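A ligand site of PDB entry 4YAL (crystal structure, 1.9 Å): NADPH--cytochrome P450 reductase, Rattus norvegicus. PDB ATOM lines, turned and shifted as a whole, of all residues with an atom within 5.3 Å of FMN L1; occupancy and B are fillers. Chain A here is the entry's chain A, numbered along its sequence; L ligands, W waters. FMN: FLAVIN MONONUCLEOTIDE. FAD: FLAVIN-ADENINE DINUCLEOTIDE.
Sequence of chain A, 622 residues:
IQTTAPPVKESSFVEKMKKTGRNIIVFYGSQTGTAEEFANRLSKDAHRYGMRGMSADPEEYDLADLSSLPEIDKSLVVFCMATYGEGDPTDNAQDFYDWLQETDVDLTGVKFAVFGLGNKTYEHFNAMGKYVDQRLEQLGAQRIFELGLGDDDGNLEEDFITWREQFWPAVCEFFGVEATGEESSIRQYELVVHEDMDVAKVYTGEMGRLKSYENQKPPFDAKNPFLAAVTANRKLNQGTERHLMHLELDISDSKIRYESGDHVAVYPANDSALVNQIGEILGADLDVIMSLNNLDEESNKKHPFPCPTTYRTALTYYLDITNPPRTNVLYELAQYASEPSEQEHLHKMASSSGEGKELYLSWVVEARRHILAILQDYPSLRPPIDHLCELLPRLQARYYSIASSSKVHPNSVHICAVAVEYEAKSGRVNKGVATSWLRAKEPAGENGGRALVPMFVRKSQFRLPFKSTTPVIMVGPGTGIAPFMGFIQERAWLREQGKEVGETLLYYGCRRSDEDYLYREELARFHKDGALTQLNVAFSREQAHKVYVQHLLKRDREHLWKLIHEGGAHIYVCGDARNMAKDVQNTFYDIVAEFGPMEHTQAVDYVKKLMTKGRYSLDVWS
The backbone NH of Ser 30 is in hydrogen-bond range of the side-chain hydroxyl of Thr 90 (3.4 Å). The backbone NH (N) of Thr 83 is in hydrogen-bond range of the backbone carbonyl oxygen (O) of Leu 117 (3.0 Å). A ring nitrogen (ND1) of His 124 is in hydrogen-bond range of the side-chain carboxylate (OE1) of Glu 86, at 3.3 Å. The backbone NH (N) of Thr 34 sits at hydrogen-bond distance from the side-chain hydroxyl (OG) of Ser 30, 3.3 Å away. The side-chain amide oxygen (OD1) of Asn 126 is in hydrogen-bond range of the backbone NH (N) of Gly 118, at 3.4 Å. The backbone NH of Leu 117 sits at hydrogen-bond distance from the side-chain amide oxygen of Asn 126. O of Gly 29 sits at hydrogen-bond distance from N of Ala 82, at 2.9 Å. The side-chain carboxylate of Asp 88 lies within hydrogen-bond range of the backbone NH of Glu 86 (3.2 Å).
The backbone carbonyl oxygen (O) of Gly 85 sits close to a nitrogen (N5) of FMN L1 (2.9 Å). Residues that only touch FMN L1: Ala 82 (3.3 Å), Tyr 84 (3.4 Å), Glu 86 (3.9 Å), Gly 118 (3.1 Å), Tyr 122 (3.4 Å), Phe 125 (3.4 Å) and Leu 156 (3.3 Å). Hydrophobic or aromatic side chains that line FMN L1: Ala 35, Ala 82, Tyr 84, Leu 117, Tyr 122, Phe 125 and Leu 156. Within 4 Å of FMN L1: Ser 30, Gln 31, Thr 32, Gly 33, Thr 34, Ala 35, Ala 82, Thr 83, Tyr 84, Gly 85, Glu 86, Gly 87, Leu 117, Gly 118, Asn 119, Tyr 122, His 124, Phe 125, Asn 126, Asp 152 and Leu 156. The nearest printed residue that does not touch FMN L1 is Thr 90 (4.3 Å).
The side-chain hydroxyl (OG) of Ser 30 is in hydrogen-bond range of an oxygen (O3P) of FMN L1. The backbone carbonyl oxygen (O) of Leu 117 lies within hydrogen-bond range of an oxygen (O2') of FMN L1 (3.2 Å). The backbone carbonyl oxygen (O) of Thr 83 is in hydrogen-bond range of an oxygen (O2') of FMN L1. An oxygen (O2P) of FMN L1 sits at hydrogen-bond distance from the backbone NH (N) of Thr 32 (3.0 Å). A nitrogen (N3) of FMN L1 sits at hydrogen-bond distance from the backbone carbonyl oxygen of His 124 (3.0 Å). OD2 of Asp 152 sits at hydrogen-bond distance from O3' of FMN L1, 3.2 Å away. N of Gln 31 lies within hydrogen-bond range of O2P of FMN L1 (2.7 Å). OG1 of Thr 32 is in hydrogen-bond range of O1P of FMN L1, at 2.5 Å. The backbone NH of Gly 87 sits at hydrogen-bond distance from an oxygen (O4) of FMN L1 (2.9 Å). The backbone NH (N) of Asn 119 is in hydrogen-bond range of an oxygen (O2) of FMN L1 (3.0 Å). An oxygen (O2) of FMN L1 sits at hydrogen-bond distance from the backbone NH (N) of Asn 126 (2.7 Å). An oxygen (O1P) of FMN L1 sits at hydrogen-bond distance from the side-chain hydroxyl (OG1) of Thr 34, 2.9 Å away. The backbone NH (N) of Thr 83 sits at hydrogen-bond distance from an oxygen (O2') of FMN L1. The backbone NH (N) of Gly 33 sits at hydrogen-bond distance from an oxygen (O1P) of FMN L1 (3.4 Å). N of Thr 34 sits at hydrogen-bond distance from O1P of FMN L1. An oxygen (O3P) of FMN L1 is in hydrogen-bond range of the backbone NH (N) of Ala 35, 2.6 Å away.
Water W5 lies within hydrogen-bond range of an oxygen (O4) of FMN L1 (2.7 Å), the backbone NH of His 124 (2.8 Å), the side-chain carboxylate of Glu 86 (2.9 Å) and the backbone NH of Gly 87 (3.4 Å). Water W4 lies within hydrogen-bond range of the side-chain carboxylate of Asp 152, an oxygen (O3') of FMN L1 and the side-chain amide nitrogen of Asn 119. Water W3 lies within hydrogen-bond range of O2P of FMN L1 (2.7 Å) and O of Thr 83 (3.0 Å). Water W1 lies within hydrogen-bond range of OG1 of Thr 34 (2.7 Å) and O4' of FMN L1 (3.0 Å).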
ATOM      1  N   GLY A  29     -25.629  11.033  -7.287  1.00  0.00           N
ATOM      2  CA  GLY A  29     -25.710   9.810  -8.085  1.00  0.00           C
ATOM      3  C   GLY A  29     -26.793   9.055  -7.361  1.00  0.00           C
ATOM      4  O   GLY A  29     -26.532   8.387  -6.362  1.00  0.00           O
ATOM      5  N   SER A  30     -28.025   9.155  -7.858  1.00  0.00           N
ATOM      6  CA  SER A  30     -29.143   8.515  -7.191  1.00  0.00           C
ATOM      7  C   SER A  30     -30.036   7.671  -8.101  1.00  0.00           C
ATOM      8  O   SER A  30     -30.310   8.038  -9.247  1.00  0.00           O
ATOM      9  CB  SER A  30     -29.992   9.608  -6.510  1.00  0.00           C
ATOM     10  OG  SER A  30     -30.885   9.046  -5.574  1.00  0.00           O
ATOM     11  N   GLN A  31     -30.485   6.533  -7.577  1.00  0.00           N
ATOM     12  CA  GLN A  31     -31.354   5.624  -8.320  1.00  0.00           C
ATOM     13  C   GLN A  31     -32.752   5.727  -7.728  1.00  0.00           C
ATOM     14  O   GLN A  31     -33.751   5.796  -8.442  1.00  0.00           O
ATOM     15  CB  GLN A  31     -30.848   4.185  -8.223  1.00  0.00           C
ATOM     16  CG  GLN A  31     -31.493   3.205  -9.206  1.00  0.00           C
ATOM     17  CD  GLN A  31     -31.159   3.526 -10.644  1.00  0.00           C
ATOM     18  OE1 GLN A  31     -30.014   3.855 -10.972  1.00  0.00           O
ATOM     19  NE2 GLN A  31     -32.152   3.415 -11.527  1.00  0.00           N
ATOM     20  N   THR A  32     -32.831   5.723  -6.398  1.00  0.00           N
ATOM     21  CA  THR A  32     -34.111   5.813  -5.717  1.00  0.00           C
ATOM     22  C   THR A  32     -34.267   7.068  -4.856  1.00  0.00           C
ATOM     23  O   THR A  32     -35.003   7.064  -3.866  1.00  0.00           O
ATOM     24  CB  THR A  32     -34.384   4.537  -4.875  1.00  0.00           C
ATOM     25  OG1 THR A  32     -33.203   4.146  -4.174  1.00  0.00           O
ATOM     26  CG2 THR A  32     -34.815   3.398  -5.801  1.00  0.00           C
ATOM     27  N   GLY A  33     -33.578   8.136  -5.253  1.00  0.00           N
ATOM     28  CA  GLY A  33     -33.692   9.416  -4.570  1.00  0.00           C
ATOM     29  C   GLY A  33     -33.025   9.714  -3.236  1.00  0.00           C
ATOM     30  O   GLY A  33     -33.097  10.851  -2.762  1.00  0.00           O
ATOM     31  N   THR A  34     -32.398   8.735  -2.609  1.00  0.00           N
ATOM     32  CA  THR A  34     -31.767   8.989  -1.313  1.00  0.00           C
ATOM     33  C   THR A  34     -30.603   9.980  -1.419  1.00  0.00           C
ATOM     34  O   THR A  34     -30.532  10.952  -0.660  1.00  0.00           O
ATOM     35  CB  THR A  34     -31.281   7.677  -0.667  1.00  0.00           C
ATOM     36  OG1 THR A  34     -32.390   6.760  -0.570  1.00  0.00           O
ATOM     37  CG2 THR A  34     -30.759   7.939   0.742  1.00  0.00           C
ATOM     38  N   ALA A  35     -29.693   9.729  -2.360  1.00  0.00           N
ATOM     39  CA  ALA A  35     -28.543  10.601  -2.563  1.00  0.00           C
ATOM     40  C   ALA A  35     -28.995  11.970  -3.045  1.00  0.00           C
ATOM     41  O   ALA A  35     -28.356  12.986  -2.760  1.00  0.00           O
ATOM     42  CB  ALA A  35     -27.566   9.975  -3.577  1.00  0.00           C
ATOM     43  N   GLU A  36     -30.094  12.006  -3.792  1.00  0.00           N
ATOM     44  CA  GLU A  36     -30.612  13.270  -4.293  1.00  0.00           C
ATOM     45  C   GLU A  36     -31.019  14.161  -3.126  1.00  0.00           C
ATOM     46  O   GLU A  36     -30.716  15.346  -3.110  1.00  0.00           O
ATOM     47  CB  GLU A  36     -31.825  13.028  -5.189  1.00  0.00           C
ATOM     48  CG  GLU A  36     -32.216  14.239  -5.992  1.00  0.00           C
ATOM     49  CD  GLU A  36     -33.483  14.000  -6.790  1.00  0.00           C
ATOM     50  OE1 GLU A  36     -33.722  12.855  -7.212  1.00  0.00           O
ATOM     51  OE2 GLU A  36     -34.232  14.973  -6.990  1.00  0.00           O
ATOM     52  N   ALA A  82     -24.495   7.099  -4.725  1.00  0.00           N
ATOM     53  CA  ALA A  82     -24.988   5.790  -4.314  1.00  0.00           C
ATOM     54  C   ALA A  82     -24.434   4.780  -5.304  1.00  0.00           C
ATOM     55  O   ALA A  82     -24.064   5.134  -6.424  1.00  0.00           O
ATOM     56  CB  ALA A  82     -26.511   5.771  -4.345  1.00  0.00           C
ATOM     57  N   THR A  83     -24.354   3.529  -4.879  1.00  0.00           N
ATOM     58  CA  THR A  83     -23.889   2.463  -5.745  1.00  0.00           C
ATOM     59  C   THR A  83     -25.136   1.677  -6.154  1.00  0.00           C
ATOM     60  O   THR A  83     -26.143   1.702  -5.450  1.00  0.00           O
ATOM     61  CB  THR A  83     -22.895   1.543  -5.000  1.00  0.00           C
ATOM     62  OG1 THR A  83     -21.739   2.307  -4.626  1.00  0.00           O
ATOM     63  CG2 THR A  83     -22.451   0.384  -5.890  1.00  0.00           C
ATOM     64  N   TYR A  84     -25.072   1.010  -7.301  1.00  0.00           N
ATOM     65  CA  TYR A  84     -26.222   0.244  -7.767  1.00  0.00           C
ATOM     66  C   TYR A  84     -25.728  -0.970  -8.532  1.00  0.00           C
ATOM     67  O   TYR A  84     -24.533  -1.126  -8.737  1.00  0.00           O
ATOM     68  CB  TYR A  84     -27.107   1.115  -8.666  1.00  0.00           C
ATOM     69  CG  TYR A  84     -28.532   0.603  -8.783  1.00  0.00           C
ATOM     70  CD1 TYR A  84     -29.362   0.556  -7.666  1.00  0.00           C
ATOM     71  CD2 TYR A  84     -29.055   0.169 -10.000  1.00  0.00           C
ATOM     72  CE1 TYR A  84     -30.675   0.085  -7.759  1.00  0.00           C
ATOM     73  CE2 TYR A  84     -30.362  -0.307 -10.101  1.00  0.00           C
ATOM     74  CZ  TYR A  84     -31.167  -0.343  -8.973  1.00  0.00           C
ATOM     75  OH  TYR A  84     -32.451  -0.828  -9.038  1.00  0.00           O
ATOM     76  N   GLY A  85     -26.654  -1.818  -8.956  1.00  0.00           N
ATOM     77  CA  GLY A  85     -26.266  -3.015  -9.682  1.00  0.00           C
ATOM     78  C   GLY A  85     -25.251  -3.792  -8.877  1.00  0.00           C
ATOM     79  O   GLY A  85     -25.490  -4.122  -7.709  1.00  0.00           O
ATOM     80  N   GLU A  86     -24.120  -4.099  -9.495  1.00  0.00           N
ATOM     81  CA  GLU A  86     -23.065  -4.832  -8.826  1.00  0.00           C
ATOM     82  C   GLU A  86     -21.805  -3.985  -8.748  1.00  0.00           C
ATOM     83  O   GLU A  86     -20.887  -4.139  -9.554  1.00  0.00           O
ATOM     84  CB  GLU A  86     -22.781  -6.139  -9.554  1.00  0.00           C
ATOM     85  CG  GLU A  86     -23.254  -7.356  -8.790  1.00  0.00           C
ATOM     86  CD  GLU A  86     -22.670  -7.387  -7.386  1.00  0.00           C
ATOM     87  OE1 GLU A  86     -21.432  -7.359  -7.267  1.00  0.00           O
ATOM     88  OE2 GLU A  86     -23.459  -7.436  -6.418  1.00  0.00           O
ATOM     89  N   GLY A  87     -21.787  -3.070  -7.784  1.00  0.00           N
ATOM     90  CA  GLY A  87     -20.648  -2.186  -7.620  1.00  0.00           C
ATOM     91  C   GLY A  87     -20.568  -1.203  -8.764  1.00  0.00           C
ATOM     92  O   GLY A  87     -19.483  -0.735  -9.112  1.00  0.00           O
ATOM     93  N   ASP A  88     -21.712  -0.866  -9.337  1.00  0.00           N
ATOM     94  CA  ASP A  88     -21.770   0.058 -10.456  1.00  0.00           C
ATOM     95  C   ASP A  88     -22.347   1.426 -10.105  1.00  0.00           C
ATOM     96  O   ASP A  88     -22.909   1.615  -9.023  1.00  0.00           O
ATOM     97  CB  ASP A  88     -22.616  -0.549 -11.594  1.00  0.00           C
ATOM     98  CG  ASP A  88     -22.026  -1.832 -12.141  1.00  0.00           C
ATOM     99  OD1 ASP A  88     -20.882  -1.797 -12.624  1.00  0.00           O
ATOM    100  OD2 ASP A  88     -22.717  -2.874 -12.089  1.00  0.00           O
ATOM    101  N   THR A  90     -24.946   4.689 -10.426  1.00  0.00           N
ATOM    102  CA  THR A  90     -26.391   4.714 -10.597  1.00  0.00           C
ATOM    103  C   THR A  90     -26.569   5.071 -12.067  1.00  0.00           C
ATOM    104  O   THR A  90     -25.638   5.558 -12.696  1.00  0.00           O
ATOM    105  CB  THR A  90     -27.051   5.792  -9.722  1.00  0.00           C
ATOM    106  OG1 THR A  90     -26.348   7.023  -9.871  1.00  0.00           O
ATOM    107  CG2 THR A  90     -27.042   5.366  -8.255  1.00  0.00           C
ATOM    108  N   LEU A 117     -23.171   6.284  -0.728  1.00  0.00           N
ATOM    109  CA  LEU A 117     -24.318   5.554  -0.203  1.00  0.00           C
ATOM    110  C   LEU A 117     -24.188   4.108  -0.687  1.00  0.00           C
ATOM    111  O   LEU A 117     -24.095   3.852  -1.883  1.00  0.00           O
ATOM    112  CB  LEU A 117     -25.641   6.132  -0.723  1.00  0.00           C
ATOM    113  CG  LEU A 117     -26.111   7.510  -0.250  1.00  0.00           C
ATOM    114  CD1 LEU A 117     -25.283   8.589  -0.929  1.00  0.00           C
ATOM    115  CD2 LEU A 117     -27.599   7.686  -0.601  1.00  0.00           C
ATOM    116  N   GLY A 118     -24.155   3.170   0.259  1.00  0.00           N
ATOM    117  CA  GLY A 118     -24.039   1.773  -0.101  1.00  0.00           C
ATOM    118  C   GLY A 118     -24.743   0.870   0.879  1.00  0.00           C
ATOM    119  O   GLY A 118     -25.601   1.314   1.652  1.00  0.00           O
ATOM    120  N   ASN A 119     -24.371  -0.397   0.857  1.00  0.00           N
ATOM    121  CA  ASN A 119     -24.967  -1.389   1.749  1.00  0.00           C
ATOM    122  C   ASN A 119     -23.922  -2.480   1.913  1.00  0.00           C
ATOM    123  O   ASN A 119     -23.548  -3.144   0.934  1.00  0.00           O
ATOM    124  CB  ASN A 119     -26.231  -1.960   1.123  1.00  0.00           C
ATOM    125  CG  ASN A 119     -26.973  -2.891   2.054  1.00  0.00           C
ATOM    126  OD1 ASN A 119     -26.357  -3.758   2.685  1.00  0.00           O
ATOM    127  ND2 ASN A 119     -28.281  -2.719   2.158  1.00  0.00           N
ATOM    128  N   LYS A 120     -23.456  -2.668   3.145  1.00  0.00           N
ATOM    129  CA  LYS A 120     -22.421  -3.662   3.430  1.00  0.00           C
ATOM    130  C   LYS A 120     -22.745  -5.105   3.085  1.00  0.00           C
ATOM    131  O   LYS A 120     -21.844  -5.936   3.012  1.00  0.00           O
ATOM    132  CB  LYS A 120     -22.014  -3.595   4.911  1.00  0.00           C
ATOM    133  CG  LYS A 120     -21.084  -2.437   5.250  1.00  0.00           C
ATOM    134  CD  LYS A 120     -20.562  -2.568   6.677  1.00  0.00           C
ATOM    135  CE  LYS A 120     -19.679  -1.398   7.058  1.00  0.00           C
ATOM    136  NZ  LYS A 120     -20.425  -0.111   6.989  1.00  0.00           N
ATOM    137  N   TYR A 122     -23.770  -6.063   0.310  1.00  0.00           N
ATOM    138  CA  TYR A 122     -23.442  -6.240  -1.104  1.00  0.00           C
ATOM    139  C   TYR A 122     -21.975  -6.542  -1.345  1.00  0.00           C
ATOM    140  O   TYR A 122     -21.103  -6.137  -0.567  1.00  0.00           O
ATOM    141  CB  TYR A 122     -23.870  -5.015  -1.915  1.00  0.00           C
ATOM    142  CG  TYR A 122     -25.354  -4.964  -2.184  1.00  0.00           C
ATOM    143  CD1 TYR A 122     -26.244  -4.521  -1.200  1.00  0.00           C
ATOM    144  CD2 TYR A 122     -25.874  -5.414  -3.390  1.00  0.00           C
ATOM    145  CE1 TYR A 122     -27.626  -4.539  -1.423  1.00  0.00           C
ATOM    146  CE2 TYR A 122     -27.252  -5.436  -3.621  1.00  0.00           C
ATOM    147  CZ  TYR A 122     -28.119  -4.999  -2.631  1.00  0.00           C
ATOM    148  OH  TYR A 122     -29.478  -5.023  -2.849  1.00  0.00           O
ATOM    149  N   HIS A 124     -19.665  -5.449  -3.494  1.00  0.00           N
ATOM    150  CA  HIS A 124     -18.782  -4.300  -3.578  1.00  0.00           C
ATOM    151  C   HIS A 124     -19.391  -3.103  -2.854  1.00  0.00           C
ATOM    152  O   HIS A 124     -20.066  -2.267  -3.450  1.00  0.00           O
ATOM    153  CB  HIS A 124     -18.519  -3.945  -5.046  1.00  0.00           C
ATOM    154  CG  HIS A 124     -17.854  -5.033  -5.815  1.00  0.00           C
ATOM    155  ND1 HIS A 124     -18.551  -5.956  -6.569  1.00  0.00           N
ATOM    156  CD2 HIS A 124     -16.541  -5.373  -5.932  1.00  0.00           C
ATOM    157  CE1 HIS A 124     -17.704  -6.808  -7.117  1.00  0.00           C
ATOM    158  NE2 HIS A 124     -16.476  -6.480  -6.745  1.00  0.00           N
ATOM    159  N   PHE A 125     -19.133  -3.027  -1.548  1.00  0.00           N
ATOM    160  CA  PHE A 125     -19.656  -1.961  -0.709  1.00  0.00           C
ATOM    161  C   PHE A 125     -19.202  -0.542  -1.079  1.00  0.00           C
ATOM    162  O   PHE A 125     -18.001  -0.244  -1.076  1.00  0.00           O
ATOM    163  CB  PHE A 125     -19.275  -2.253   0.737  1.00  0.00           C
ATOM    164  CG  PHE A 125     -19.647  -1.172   1.697  1.00  0.00           C
ATOM    165  CD1 PHE A 125     -20.962  -0.730   1.802  1.00  0.00           C
ATOM    166  CD2 PHE A 125     -18.677  -0.586   2.509  1.00  0.00           C
ATOM    167  CE1 PHE A 125     -21.316   0.266   2.692  1.00  0.00           C
ATOM    168  CE2 PHE A 125     -19.027   0.419   3.410  1.00  0.00           C
ATOM    169  CZ  PHE A 125     -20.345   0.845   3.509  1.00  0.00           C
ATOM    170  N   ASN A 126     -20.159   0.318  -1.392  1.00  0.00           N
ATOM    171  CA  ASN A 126     -19.872   1.705  -1.747  1.00  0.00           C
ATOM    172  C   ASN A 126     -18.844   1.880  -2.851  1.00  0.00           C
ATOM    173  O   ASN A 126     -18.092   2.852  -2.871  1.00  0.00           O
ATOM    174  CB  ASN A 126     -19.394   2.475  -0.500  1.00  0.00           C
ATOM    175  CG  ASN A 126     -20.478   3.355   0.088  1.00  0.00           C
ATOM    176  OD1 ASN A 126     -21.070   4.178  -0.608  1.00  0.00           O
ATOM    177  ND2 ASN A 126     -20.739   3.201   1.388  1.00  0.00           N
ATOM    178  N   ALA A 127     -18.838   0.951  -3.803  1.00  0.00           N
ATOM    179  CA  ALA A 127     -17.895   0.993  -4.908  1.00  0.00           C
ATOM    180  C   ALA A 127     -17.850   2.339  -5.636  1.00  0.00           C
ATOM    181  O   ALA A 127     -16.769   2.845  -5.929  1.00  0.00           O
ATOM    182  CB  ALA A 127     -18.211  -0.124  -5.907  1.00  0.00           C
ATOM    183  N   ASP A 152     -26.599   1.462   4.253  1.00  0.00           N
ATOM    184  CA  ASP A 152     -28.041   1.271   4.332  1.00  0.00           C
ATOM    185  C   ASP A 152     -28.432   0.006   5.086  1.00  0.00           C
ATOM    186  O   ASP A 152     -29.616  -0.197   5.389  1.00  0.00           O
ATOM    187  CB  ASP A 152     -28.631   1.276   2.912  1.00  0.00           C
ATOM    188  CG  ASP A 152     -30.124   1.534   2.903  1.00  0.00           C
ATOM    189  OD1 ASP A 152     -30.615   2.335   3.727  1.00  0.00           O
ATOM    190  OD2 ASP A 152     -30.819   0.937   2.054  1.00  0.00           O
ATOM    191  N   LEU A 156     -28.426   4.475   7.329  1.00  0.00           N
ATOM    192  CA  LEU A 156     -27.809   5.431   6.419  1.00  0.00           C
ATOM    193  C   LEU A 156     -27.992   6.864   6.875  1.00  0.00           C
ATOM    194  O   LEU A 156     -27.056   7.669   6.800  1.00  0.00           O
ATOM    195  CB  LEU A 156     -28.388   5.244   5.019  1.00  0.00           C
ATOM    196  CG  LEU A 156     -27.895   6.191   3.921  1.00  0.00           C
ATOM    197  CD1 LEU A 156     -26.390   6.039   3.748  1.00  0.00           C
ATOM    198  CD2 LEU A 156     -28.628   5.883   2.617  1.00  0.00           C
ATOM    199  N   VAL A 620     -30.896 -10.062  -6.217  1.00  0.00           N
ATOM    200  CA  VAL A 620     -31.340 -10.105  -4.838  1.00  0.00           C
ATOM    201  C   VAL A 620     -31.691  -8.704  -4.367  1.00  0.00           C
ATOM    202  O   VAL A 620     -31.092  -7.720  -4.800  1.00  0.00           O
ATOM    203  CB  VAL A 620     -30.257 -10.722  -3.938  1.00  0.00           C
ATOM    204  CG1 VAL A 620     -30.010 -12.171  -4.340  1.00  0.00           C
ATOM    205  CG2 VAL A 620     -28.979  -9.920  -4.050  1.00  0.00           C
HETATM  206  N1  FMN L   1     -24.781  -0.739  -2.284  1.00  0.00           N
HETATM  207  C2  FMN L   1     -23.462  -1.001  -2.378  1.00  0.00           C
HETATM  208  O2  FMN L   1     -22.661  -0.564  -1.546  1.00  0.00           O
HETATM  209  N3  FMN L   1     -23.051  -1.768  -3.456  1.00  0.00           N
HETATM  210  C4  FMN L   1     -23.849  -2.315  -4.463  1.00  0.00           C
HETATM  211  O4  FMN L   1     -23.252  -2.969  -5.322  1.00  0.00           O
HETATM  212  C4A FMN L   1     -25.242  -2.071  -4.367  1.00  0.00           C
HETATM  213  N5  FMN L   1     -26.081  -2.623  -5.358  1.00  0.00           N
HETATM  214  C5A FMN L   1     -27.436  -2.356  -5.182  1.00  0.00           C
HETATM  215  C6  FMN L   1     -28.311  -2.942  -6.163  1.00  0.00           C
HETATM  216  C7  FMN L   1     -29.716  -2.755  -6.093  1.00  0.00           C
HETATM  217  C7M FMN L   1     -30.535  -3.446  -7.214  1.00  0.00           C
HETATM  218  C8  FMN L   1     -30.331  -1.935  -4.997  1.00  0.00           C
HETATM  219  C8M FMN L   1     -31.676  -1.686  -4.830  1.00  0.00           C
HETATM  220  C9  FMN L   1     -29.495  -1.363  -4.048  1.00  0.00           C
HETATM  221  C9A FMN L   1     -28.041  -1.545  -4.100  1.00  0.00           C
HETATM  222  N10 FMN L   1     -27.086  -0.987  -3.117  1.00  0.00           N
HETATM  223  C10 FMN L   1     -25.645  -1.259  -3.244  1.00  0.00           C
HETATM  224  C1' FMN L   1     -27.574  -0.180  -2.007  1.00  0.00           C
HETATM  225  C2' FMN L   1     -27.738   1.342  -2.332  1.00  0.00           C
HETATM  226  O2' FMN L   1     -26.423   1.893  -2.753  1.00  0.00           O
HETATM  227  C3' FMN L   1     -28.259   2.080  -1.106  1.00  0.00           C
HETATM  228  O3' FMN L   1     -29.549   1.504  -0.775  1.00  0.00           O
HETATM  229  C4' FMN L   1     -28.363   3.592  -1.453  1.00  0.00           C
HETATM  230  O4' FMN L   1     -28.847   4.139  -0.189  1.00  0.00           O
HETATM  231  C5' FMN L   1     -29.412   3.929  -2.494  1.00  0.00           C
HETATM  232  O5' FMN L   1     -29.423   5.373  -2.830  1.00  0.00           O
HETATM  233  P   FMN L   1     -30.391   6.051  -3.868  1.00  0.00           P
HETATM  234  O1P FMN L   1     -31.787   6.021  -3.342  1.00  0.00           O
HETATM  235  O2P FMN L   1     -30.053   5.354  -5.220  1.00  0.00           O
HETATM  236  O3P FMN L   1     -29.880   7.569  -3.812  1.00  0.00           O
HETATM  237  PA  FAD L   2     -43.014  -0.396   0.570  1.00  0.00           P
HETATM  238  O1A FAD L   2     -44.116   0.542   0.876  1.00  0.00           O
HETATM  239  O2A FAD L   2     -41.904   0.064  -0.316  1.00  0.00           O
HETATM  240  O5B FAD L   2     -42.367  -0.902   1.951  1.00  0.00           O
HETATM  241  C5B FAD L   2     -41.150  -1.650   1.931  1.00  0.00           C
HETATM  242  C4B FAD L   2     -40.495  -1.544   3.310  1.00  0.00           C
HETATM  243  O4B FAD L   2     -41.364  -2.073   4.324  1.00  0.00           O
HETATM  244  C3B FAD L   2     -39.297  -2.464   3.415  1.00  0.00           C
HETATM  245  O3B FAD L   2     -38.183  -1.841   2.743  1.00  0.00           O
HETATM  246  C2B FAD L   2     -39.090  -2.380   4.913  1.00  0.00           C
HETATM  247  O2B FAD L   2     -38.420  -1.145   5.244  1.00  0.00           O
HETATM  248  C1B FAD L   2     -40.516  -2.347   5.448  1.00  0.00           C
HETATM  249  N9A FAD L   2     -40.940  -3.675   5.960  1.00  0.00           N
HETATM  250  C8A FAD L   2     -41.436  -4.795   5.141  1.00  0.00           C
HETATM  251  N7A FAD L   2     -41.768  -5.772   6.190  1.00  0.00           N
HETATM  252  C5A FAD L   2     -41.433  -5.271   7.374  1.00  0.00           C
HETATM  253  C6A FAD L   2     -41.564  -5.814   8.573  1.00  0.00           C
HETATM  254  N6A FAD L   2     -42.187  -6.988   8.618  1.00  0.00           N
HETATM  255  N1A FAD L   2     -41.197  -5.181   9.695  1.00  0.00           N
HETATM  256  C2A FAD L   2     -40.653  -3.895   9.593  1.00  0.00           C
HETATM  257  N3A FAD L   2     -40.527  -3.345   8.317  1.00  0.00           N
HETATM  258  C4A FAD L   2     -40.918  -4.048   7.238  1.00  0.00           C
HETATM  259  N1  FAD L   2     -40.264  -7.944  -4.822  1.00  0.00           N
HETATM  260  C2  FAD L   2     -41.105  -9.003  -5.191  1.00  0.00           C
HETATM  261  O2  FAD L   2     -41.986  -9.368  -4.414  1.00  0.00           O
HETATM  262  N3  FAD L   2     -40.889  -9.654  -6.408  1.00  0.00           N
HETATM  263  C4  FAD L   2     -39.839  -9.275  -7.243  1.00  0.00           C
HETATM  264  O4  FAD L   2     -39.715  -9.819  -8.346  1.00  0.00           O
HETATM  265  C4X FAD L   2     -38.991  -8.237  -6.870  1.00  0.00           C
HETATM  266  N5  FAD L   2     -37.874  -7.979  -7.555  1.00  0.00           N
HETATM  267  C5X FAD L   2     -37.072  -6.970  -7.182  1.00  0.00           C
HETATM  268  C6  FAD L   2     -35.982  -6.626  -7.967  1.00  0.00           C
HETATM  269  C7  FAD L   2     -35.200  -5.518  -7.643  1.00  0.00           C
HETATM  270  C7M FAD L   2     -34.132  -5.173  -8.458  1.00  0.00           C
HETATM  271  C8  FAD L   2     -35.522  -4.753  -6.529  1.00  0.00           C
HETATM  272  C8M FAD L   2     -34.768  -3.635  -6.202  1.00  0.00           C
HETATM  273  C9  FAD L   2     -36.617  -5.093  -5.736  1.00  0.00           C
HETATM  274  C9A FAD L   2     -37.410  -6.180  -6.082  1.00  0.00           C
HETATM  275  N10 FAD L   2     -38.521  -6.459  -5.392  1.00  0.00           N
HETATM  276  C10 FAD L   2     -39.207  -7.577  -5.659  1.00  0.00           C
HETATM  277  C1' FAD L   2     -38.933  -5.649  -4.218  1.00  0.00           C
HETATM  278  C2' FAD L   2     -39.950  -4.594  -4.682  1.00  0.00           C
HETATM  279  O2' FAD L   2     -39.297  -3.685  -5.577  1.00  0.00           O
HETATM  280  C3' FAD L   2     -40.549  -3.807  -3.512  1.00  0.00           C
HETATM  281  O3' FAD L   2     -39.493  -3.308  -2.681  1.00  0.00           O
HETATM  282  C4' FAD L   2     -41.488  -4.690  -2.678  1.00  0.00           C
HETATM  283  O4' FAD L   2     -42.502  -5.254  -3.520  1.00  0.00           O
HETATM  284  C5' FAD L   2     -42.149  -3.826  -1.599  1.00  0.00           C
HETATM  285  O5' FAD L   2     -42.752  -2.688  -2.214  1.00  0.00           O
HETATM  286  P   FAD L   2     -44.032  -1.951  -1.574  1.00  0.00           P
HETATM  287  O1P FAD L   2     -45.191  -2.860  -1.613  1.00  0.00           O
HETATM  288  O2P FAD L   2     -44.160  -0.623  -2.232  1.00  0.00           O
HETATM  289  O3P FAD L   2     -43.625  -1.752  -0.027  1.00  0.00           O
HETATM  290  O   HOH W   1     -31.707   4.340   0.531  1.00  0.00           O
HETATM  291  O   HOH W   2     -33.716   0.229  -6.485  1.00  0.00           O
HETATM  292  O   HOH W   3     -28.858   2.939  -5.755  1.00  0.00           O
HETATM  293  O   HOH W   4     -29.878  -0.920   0.415  1.00  0.00           O
HETATM  294  O   HOH W   5     -21.937  -5.308  -5.208  1.00  0.00           O
HETATM  295  O   HOH W   6     -31.912   0.970  -2.232  1.00  0.00           O
